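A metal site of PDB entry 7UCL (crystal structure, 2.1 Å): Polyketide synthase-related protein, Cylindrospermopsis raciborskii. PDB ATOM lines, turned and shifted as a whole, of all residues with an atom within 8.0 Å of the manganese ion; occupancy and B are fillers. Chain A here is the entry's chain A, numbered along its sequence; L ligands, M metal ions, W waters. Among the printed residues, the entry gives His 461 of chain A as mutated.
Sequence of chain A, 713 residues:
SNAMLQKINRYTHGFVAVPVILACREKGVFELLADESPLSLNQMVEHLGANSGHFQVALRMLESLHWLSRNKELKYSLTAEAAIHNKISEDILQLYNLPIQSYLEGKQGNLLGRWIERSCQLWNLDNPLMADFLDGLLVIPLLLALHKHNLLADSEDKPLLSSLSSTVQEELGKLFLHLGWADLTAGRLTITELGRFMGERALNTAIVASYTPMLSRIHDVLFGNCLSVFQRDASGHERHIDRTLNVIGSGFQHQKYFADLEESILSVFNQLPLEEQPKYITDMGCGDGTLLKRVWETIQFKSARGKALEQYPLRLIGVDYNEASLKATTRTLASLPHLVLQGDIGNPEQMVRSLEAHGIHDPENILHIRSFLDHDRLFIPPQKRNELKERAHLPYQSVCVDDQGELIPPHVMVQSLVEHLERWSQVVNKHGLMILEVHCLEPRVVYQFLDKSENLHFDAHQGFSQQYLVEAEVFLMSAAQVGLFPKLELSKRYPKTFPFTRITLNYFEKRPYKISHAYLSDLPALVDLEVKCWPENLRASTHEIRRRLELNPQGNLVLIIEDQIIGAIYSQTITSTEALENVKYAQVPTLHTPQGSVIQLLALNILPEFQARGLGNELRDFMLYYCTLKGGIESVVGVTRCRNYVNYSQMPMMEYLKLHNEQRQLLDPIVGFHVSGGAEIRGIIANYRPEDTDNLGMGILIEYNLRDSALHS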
ATOM      1  N   ILE A 207      16.164   0.764  33.878  1.00  0.00           N
ATOM      2  CA  ILE A 207      15.185  -0.166  33.356  1.00  0.00           C
ATOM      3  C   ILE A 207      14.704  -1.130  34.449  1.00  0.00           C
ATOM      4  O   ILE A 207      13.497  -1.294  34.645  1.00  0.00           O
ATOM      5  CB  ILE A 207      15.731  -0.909  32.123  1.00  0.00           C
ATOM      6  CG1 ILE A 207      15.644   0.008  30.891  1.00  0.00           C
ATOM      7  CG2 ILE A 207      14.927  -2.142  31.861  1.00  0.00           C
ATOM      8  CD1 ILE A 207      16.432  -0.489  29.697  1.00  0.00           C
ATOM      9  N   TYR A 211      10.576  -1.315  36.567  1.00  0.00           N
ATOM     10  CA  TYR A 211       9.732  -2.455  36.905  1.00  0.00           C
ATOM     11  C   TYR A 211       9.419  -2.586  38.418  1.00  0.00           C
ATOM     12  O   TYR A 211       8.836  -3.595  38.826  1.00  0.00           O
ATOM     13  CB  TYR A 211      10.384  -3.741  36.394  1.00  0.00           C
ATOM     14  CG  TYR A 211      10.245  -3.866  34.899  1.00  0.00           C
ATOM     15  CD1 TYR A 211       9.020  -4.179  34.353  1.00  0.00           C
ATOM     16  CD2 TYR A 211      11.323  -3.602  34.039  1.00  0.00           C
ATOM     17  CE1 TYR A 211       8.852  -4.274  32.948  1.00  0.00           C
ATOM     18  CE2 TYR A 211      11.155  -3.697  32.633  1.00  0.00           C
ATOM     19  CZ  TYR A 211       9.916  -4.040  32.112  1.00  0.00           C
ATOM     20  OH  TYR A 211       9.706  -4.124  30.750  1.00  0.00           O
ATOM     21  N   ARG A 243       6.572   3.920  32.887  1.00  0.00           N
ATOM     22  CA  ARG A 243       6.996   3.919  31.485  1.00  0.00           C
ATOM     23  C   ARG A 243       7.963   5.057  31.174  1.00  0.00           C
ATOM     24  O   ARG A 243       8.822   4.906  30.312  1.00  0.00           O
ATOM     25  CB  ARG A 243       5.784   3.953  30.550  1.00  0.00           C
ATOM     26  CG  ARG A 243       6.091   3.991  29.025  1.00  0.00           C
ATOM     27  CD  ARG A 243       7.063   2.901  28.543  1.00  0.00           C
ATOM     28  NE  ARG A 243       6.457   1.571  28.601  1.00  0.00           N
ATOM     29  CZ  ARG A 243       7.064   0.432  28.304  1.00  0.00           C
ATOM     30  NH1 ARG A 243       8.356   0.393  27.990  1.00  0.00           N
ATOM     31  NH2 ARG A 243       6.364  -0.698  28.313  1.00  0.00           N
ATOM     32  N   ASN A 246      11.348   3.984  32.263  1.00  0.00           N
ATOM     33  CA  ASN A 246      11.764   2.910  31.386  1.00  0.00           C
ATOM     34  C   ASN A 246      12.333   3.455  30.078  1.00  0.00           C
ATOM     35  O   ASN A 246      13.379   2.997  29.613  1.00  0.00           O
ATOM     36  CB  ASN A 246      10.575   1.969  31.137  1.00  0.00           C
ATOM     37  CG  ASN A 246      10.954   0.750  30.297  1.00  0.00           C
ATOM     38  OD1 ASN A 246      10.577   0.657  29.135  1.00  0.00           O
ATOM     39  ND2 ASN A 246      11.668  -0.181  30.900  1.00  0.00           N
ATOM     40  N   SER A 250      15.909   2.807  28.416  1.00  0.00           N
ATOM     41  CA  SER A 250      16.138   2.245  27.084  1.00  0.00           C
ATOM     42  C   SER A 250      17.047   3.146  26.260  1.00  0.00           C
ATOM     43  O   SER A 250      18.014   2.679  25.632  1.00  0.00           O
ATOM     44  CB  SER A 250      14.820   2.075  26.339  1.00  0.00           C
ATOM     45  OG  SER A 250      13.974   1.140  26.956  1.00  0.00           O
ATOM     46  N   HIS A 254      20.571   1.925  24.768  1.00  0.00           N
ATOM     47  CA  HIS A 254      20.679   1.559  23.360  1.00  0.00           C
ATOM     48  C   HIS A 254      21.678   2.429  22.573  1.00  0.00           C
ATOM     49  O   HIS A 254      21.933   2.120  21.409  1.00  0.00           O
ATOM     50  CB  HIS A 254      19.310   1.622  22.682  1.00  0.00           C
ATOM     51  CG  HIS A 254      18.296   0.687  23.274  1.00  0.00           C
ATOM     52  ND1 HIS A 254      16.936   0.882  23.148  1.00  0.00           N
ATOM     53  CD2 HIS A 254      18.442  -0.438  24.021  1.00  0.00           C
ATOM     54  CE1 HIS A 254      16.282  -0.086  23.772  1.00  0.00           C
ATOM     55  NE2 HIS A 254      17.180  -0.894  24.316  1.00  0.00           N
ATOM     56  N   PHE A 372      15.536  -3.325  18.900  1.00  0.00           N
ATOM     57  CA  PHE A 372      15.004  -3.883  20.143  1.00  0.00           C
ATOM     58  C   PHE A 372      13.480  -3.789  20.176  1.00  0.00           C
ATOM     59  O   PHE A 372      12.902  -3.235  21.093  1.00  0.00           O
ATOM     60  CB  PHE A 372      15.659  -3.206  21.359  1.00  0.00           C
ATOM     61  CG  PHE A 372      17.162  -3.222  21.289  1.00  0.00           C
ATOM     62  CD1 PHE A 372      17.848  -4.419  21.372  1.00  0.00           C
ATOM     63  CD2 PHE A 372      17.879  -2.048  21.093  1.00  0.00           C
ATOM     64  CE1 PHE A 372      19.243  -4.459  21.276  1.00  0.00           C
ATOM     65  CE2 PHE A 372      19.267  -2.069  21.028  1.00  0.00           C
ATOM     66  CZ  PHE A 372      19.949  -3.280  21.109  1.00  0.00           C
ATOM     67  N   LEU A 373      12.834  -4.346  19.161  1.00  0.00           N
ATOM     68  CA  LEU A 373      11.395  -4.183  19.128  1.00  0.00           C
ATOM     69  C   LEU A 373      10.626  -5.420  18.708  1.00  0.00           C
ATOM     70  O   LEU A 373       9.460  -5.540  19.093  1.00  0.00           O
ATOM     71  CB  LEU A 373      11.023  -3.010  18.214  1.00  0.00           C
ATOM     72  CG  LEU A 373       9.583  -2.506  18.240  1.00  0.00           C
ATOM     73  CD1 LEU A 373       9.135  -2.063  19.624  1.00  0.00           C
ATOM     74  CD2 LEU A 373       9.410  -1.362  17.252  1.00  0.00           C
ATOM     75  N   HIS A 375      10.766  -8.379  19.822  1.00  0.00           N
ATOM     76  CA  HIS A 375      10.363  -9.095  21.033  1.00  0.00           C
ATOM     77  C   HIS A 375       9.207  -8.423  21.777  1.00  0.00           C
ATOM     78  O   HIS A 375       8.612  -9.039  22.680  1.00  0.00           O
ATOM     79  CB  HIS A 375      11.563  -9.260  21.971  1.00  0.00           C
ATOM     80  CG  HIS A 375      11.931  -8.001  22.698  1.00  0.00           C
ATOM     81  ND1 HIS A 375      12.913  -7.151  22.265  1.00  0.00           N
ATOM     82  CD2 HIS A 375      11.427  -7.463  23.845  1.00  0.00           C
ATOM     83  CE1 HIS A 375      13.001  -6.122  23.101  1.00  0.00           C
ATOM     84  NE2 HIS A 375      12.098  -6.280  24.052  1.00  0.00           N
ATOM     85  N   ASP A 376       8.870  -7.196  21.432  1.00  0.00           N
ATOM     86  CA  ASP A 376       7.902  -6.434  22.206  1.00  0.00           C
ATOM     87  C   ASP A 376       6.667  -6.184  21.352  1.00  0.00           C
ATOM     88  O   ASP A 376       6.221  -5.038  21.222  1.00  0.00           O
ATOM     89  CB  ASP A 376       8.545  -5.116  22.670  1.00  0.00           C
ATOM     90  CG  ASP A 376       7.724  -4.376  23.720  1.00  0.00           C
ATOM     91  OD1 ASP A 376       6.676  -4.875  24.169  1.00  0.00           O
ATOM     92  OD2 ASP A 376       8.140  -3.251  24.071  1.00  0.00           O
ATOM     93  N   ARG A 377       6.140  -7.234  20.749  1.00  0.00           N
ATOM     94  CA  ARG A 377       5.033  -7.154  19.810  1.00  0.00           C
ATOM     95  C   ARG A 377       3.810  -7.827  20.428  1.00  0.00           C
ATOM     96  O   ARG A 377       3.893  -8.531  21.426  1.00  0.00           O
ATOM     97  CB  ARG A 377       5.396  -7.837  18.483  1.00  0.00           C
ATOM     98  CG  ARG A 377       5.279  -9.356  18.501  1.00  0.00           C
ATOM     99  CD  ARG A 377       5.855 -10.038  17.209  1.00  0.00           C
ATOM    100  NE  ARG A 377       5.813 -11.505  17.321  1.00  0.00           N
ATOM    101  CZ  ARG A 377       6.784 -12.251  17.857  1.00  0.00           C
ATOM    102  NH1 ARG A 377       7.941 -11.713  18.249  1.00  0.00           N
ATOM    103  NH2 ARG A 377       6.601 -13.555  17.988  1.00  0.00           N
ATOM    104  N   GLU A 437      18.581  -6.545  17.860  1.00  0.00           N
ATOM    105  CA  GLU A 437      17.647  -7.289  18.717  1.00  0.00           C
ATOM    106  C   GLU A 437      18.396  -7.926  19.886  1.00  0.00           C
ATOM    107  O   GLU A 437      19.610  -8.120  19.857  1.00  0.00           O
ATOM    108  CB  GLU A 437      16.871  -8.337  17.906  1.00  0.00           C
ATOM    109  CG  GLU A 437      15.825  -9.175  18.718  1.00  0.00           C
ATOM    110  CD  GLU A 437      14.667  -8.369  19.374  1.00  0.00           C
ATOM    111  OE1 GLU A 437      14.874  -7.367  20.130  1.00  0.00           O
ATOM    112  OE2 GLU A 437      13.511  -8.780  19.151  1.00  0.00           O
ATOM    113  N   VAL A 438      17.647  -8.215  20.958  1.00  0.00           N
ATOM    114  CA  VAL A 438      18.178  -8.754  22.215  1.00  0.00           C
ATOM    115  C   VAL A 438      17.571 -10.141  22.390  1.00  0.00           C
ATOM    116  O   VAL A 438      16.428 -10.410  21.970  1.00  0.00           O
ATOM    117  CB  VAL A 438      17.900  -7.798  23.417  1.00  0.00           C
ATOM    118  CG1 VAL A 438      16.420  -7.520  23.604  1.00  0.00           C
ATOM    119  CG2 VAL A 438      18.541  -8.311  24.772  1.00  0.00           C
ATOM    120  N   PHE A 458      17.430  -9.358  33.213  1.00  0.00           N
ATOM    121  CA  PHE A 458      16.765  -8.869  31.994  1.00  0.00           C
ATOM    122  C   PHE A 458      15.771  -9.888  31.448  1.00  0.00           C
ATOM    123  O   PHE A 458      14.620  -9.546  31.168  1.00  0.00           O
ATOM    124  CB  PHE A 458      17.777  -8.517  30.903  1.00  0.00           C
ATOM    125  CG  PHE A 458      17.160  -7.808  29.709  1.00  0.00           C
ATOM    126  CD1 PHE A 458      16.971  -6.431  29.722  1.00  0.00           C
ATOM    127  CD2 PHE A 458      16.748  -8.523  28.582  1.00  0.00           C
ATOM    128  CE1 PHE A 458      16.402  -5.764  28.647  1.00  0.00           C
ATOM    129  CE2 PHE A 458      16.188  -7.863  27.487  1.00  0.00           C
ATOM    130  CZ  PHE A 458      15.999  -6.475  27.522  1.00  0.00           C
ATOM    131  N   HIS A 461      12.511 -10.023  33.676  1.00  0.00           N
ATOM    132  CA  HIS A 461      11.454  -9.027  33.635  1.00  0.00           C
ATOM    133  C   HIS A 461      10.851  -8.891  32.244  1.00  0.00           C
ATOM    134  O   HIS A 461       9.719  -8.402  32.119  1.00  0.00           O
ATOM    135  CB  HIS A 461      11.874  -7.637  34.171  1.00  0.00           C
ATOM    136  CG  HIS A 461      13.012  -6.953  33.454  1.00  0.00           C
ATOM    137  ND1 HIS A 461      12.967  -6.583  32.128  1.00  0.00           N
ATOM    138  CD2 HIS A 461      14.185  -6.463  33.926  1.00  0.00           C
ATOM    139  CE1 HIS A 461      14.083  -5.967  31.800  1.00  0.00           C
ATOM    140  NE2 HIS A 461      14.844  -5.870  32.880  1.00  0.00           N
ATOM    141  N   GLN A 462      11.542  -9.349  31.198  1.00  0.00           N
ATOM    142  CA  GLN A 462      10.871  -9.478  29.897  1.00  0.00           C
ATOM    143  C   GLN A 462       9.863 -10.616  29.932  1.00  0.00           C
ATOM    144  O   GLN A 462       8.767 -10.495  29.381  1.00  0.00           O
ATOM    145  CB  GLN A 462      11.887  -9.703  28.783  1.00  0.00           C
ATOM    146  CG  GLN A 462      12.989  -8.628  28.699  1.00  0.00           C
ATOM    147  CD  GLN A 462      12.439  -7.289  28.271  1.00  0.00           C
ATOM    148  OE1 GLN A 462      12.124  -7.076  27.085  1.00  0.00           O
ATOM    149  NE2 GLN A 462      12.296  -6.386  29.217  1.00  0.00           N
ATOM    150  N   SER A 465       6.718  -9.495  32.029  1.00  0.00           N
ATOM    151  CA  SER A 465       5.938  -8.452  31.362  1.00  0.00           C
ATOM    152  C   SER A 465       5.431  -8.879  29.970  1.00  0.00           C
ATOM    153  O   SER A 465       5.023  -8.011  29.189  1.00  0.00           O
ATOM    154  CB  SER A 465       6.739  -7.142  31.272  1.00  0.00           C
ATOM    155  OG  SER A 465       7.946  -7.297  30.515  1.00  0.00           O
ATOM    156  N   GLN A 467       6.795 -10.160  27.215  1.00  0.00           N
ATOM    157  CA  GLN A 467       7.590  -9.937  26.022  1.00  0.00           C
ATOM    158  C   GLN A 467       8.337 -11.228  25.686  1.00  0.00           C
ATOM    159  O   GLN A 467       8.394 -12.162  26.507  1.00  0.00           O
ATOM    160  CB  GLN A 467       8.542  -8.749  26.217  1.00  0.00           C
ATOM    161  CG  GLN A 467       7.829  -7.451  26.541  1.00  0.00           C
ATOM    162  CD  GLN A 467       8.788  -6.304  26.878  1.00  0.00           C
ATOM    163  OE1 GLN A 467       9.523  -5.805  26.033  1.00  0.00           O
ATOM    164  NE2 GLN A 467       8.775  -5.887  28.137  1.00  0.00           N
ATOM    165  N   TYR A 468       8.861 -11.311  24.461  1.00  0.00           N
ATOM    166  CA  TYR A 468       9.114 -12.609  23.812  1.00  0.00           C
ATOM    167  C   TYR A 468      10.536 -12.715  23.282  1.00  0.00           C
ATOM    168  O   TYR A 468      10.763 -12.561  22.072  1.00  0.00           O
ATOM    169  CB  TYR A 468       8.072 -12.825  22.668  1.00  0.00           C
ATOM    170  CG  TYR A 468       6.639 -12.634  23.113  1.00  0.00           C
ATOM    171  CD1 TYR A 468       6.135 -13.302  24.256  1.00  0.00           C
ATOM    172  CD2 TYR A 468       5.812 -11.765  22.447  1.00  0.00           C
ATOM    173  CE1 TYR A 468       4.820 -13.116  24.664  1.00  0.00           C
ATOM    174  CE2 TYR A 468       4.499 -11.566  22.867  1.00  0.00           C
ATOM    175  CZ  TYR A 468       4.012 -12.236  23.952  1.00  0.00           C
ATOM    176  OH  TYR A 468       2.711 -12.020  24.335  1.00  0.00           O
ATOM    177  N   LEU A 469      11.471 -13.104  24.138  1.00  0.00           N
ATOM    178  CA  LEU A 469      12.851 -13.289  23.745  1.00  0.00           C
ATOM    179  C   LEU A 469      13.078 -14.715  23.271  1.00  0.00           C
ATOM    180  O   LEU A 469      12.506 -15.672  23.832  1.00  0.00           O
ATOM    181  CB  LEU A 469      13.807 -12.984  24.901  1.00  0.00           C
ATOM    182  CG  LEU A 469      13.711 -11.624  25.580  1.00  0.00           C
ATOM    183  CD1 LEU A 469      14.772 -11.557  26.650  1.00  0.00           C
ATOM    184  CD2 LEU A 469      13.959 -10.513  24.577  1.00  0.00           C
HETATM  185  C1  LIG L   1      12.775  -2.354  27.484  1.00  0.00           C
HETATM  186  C2  LIG L   1      11.726  -3.171  28.267  1.00  0.00           C
HETATM  187  C3  LIG L   1      13.698  -3.198  26.568  1.00  0.00           C
HETATM  188  O1  LIG L   1      11.035  -3.946  27.588  1.00  0.00           O
HETATM  189  O2  LIG L   1      11.635  -3.012  29.511  1.00  0.00           O
HETATM  190  O3  LIG L   1      13.260  -4.177  25.879  1.00  0.00           O
HETATM  191  O4  LIG L   1      14.888  -2.814  26.589  1.00  0.00           O
HETATM  192 MN    MN M   1      11.591  -5.116  25.928  1.00  0.00          MN
HETATM  193  O   HOH W   1      10.698  -3.499  24.963  1.00  0.00           O
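The side-chain hydroxyl (OG) of Ser 465 sits at hydrogen-bond distance from the side-chain amide nitrogen (NE2) of Gln 467, 2.9 Å away.
The side-chain carboxylate (OE2) of Glu 437 is in hydrogen-bond range of the backbone NH (N) of His 375 (2.9 Å).
The side-chain amide nitrogen (NE2) of Gln 467 lies within hydrogen-bond range of the side-chain hydroxyl (OH) of Tyr 211 (3.3 Å).
The backbone carbonyl oxygen (O) of Gln 462 is in hydrogen-bond range of the side-chain hydroxyl (OG) of Ser 465, 3.5 Å away.
The backbone carbonyl oxygen of His 375 is in hydrogen-bond range of the backbone NH of Tyr 468.
NE2 of Gln 462 sits at hydrogen-bond distance from ND1 of His 461, at 3.0 Å.
The manganese ion is bound by O3 of the ligand (1.9 Å), water W1 (2.1 Å), O1 of the ligand (2.1 Å), OE1 of Gln 467 (2.2 Å), NE2 of His 375 (2.3 Å) and OE1 of Gln 462 (2.3 Å).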
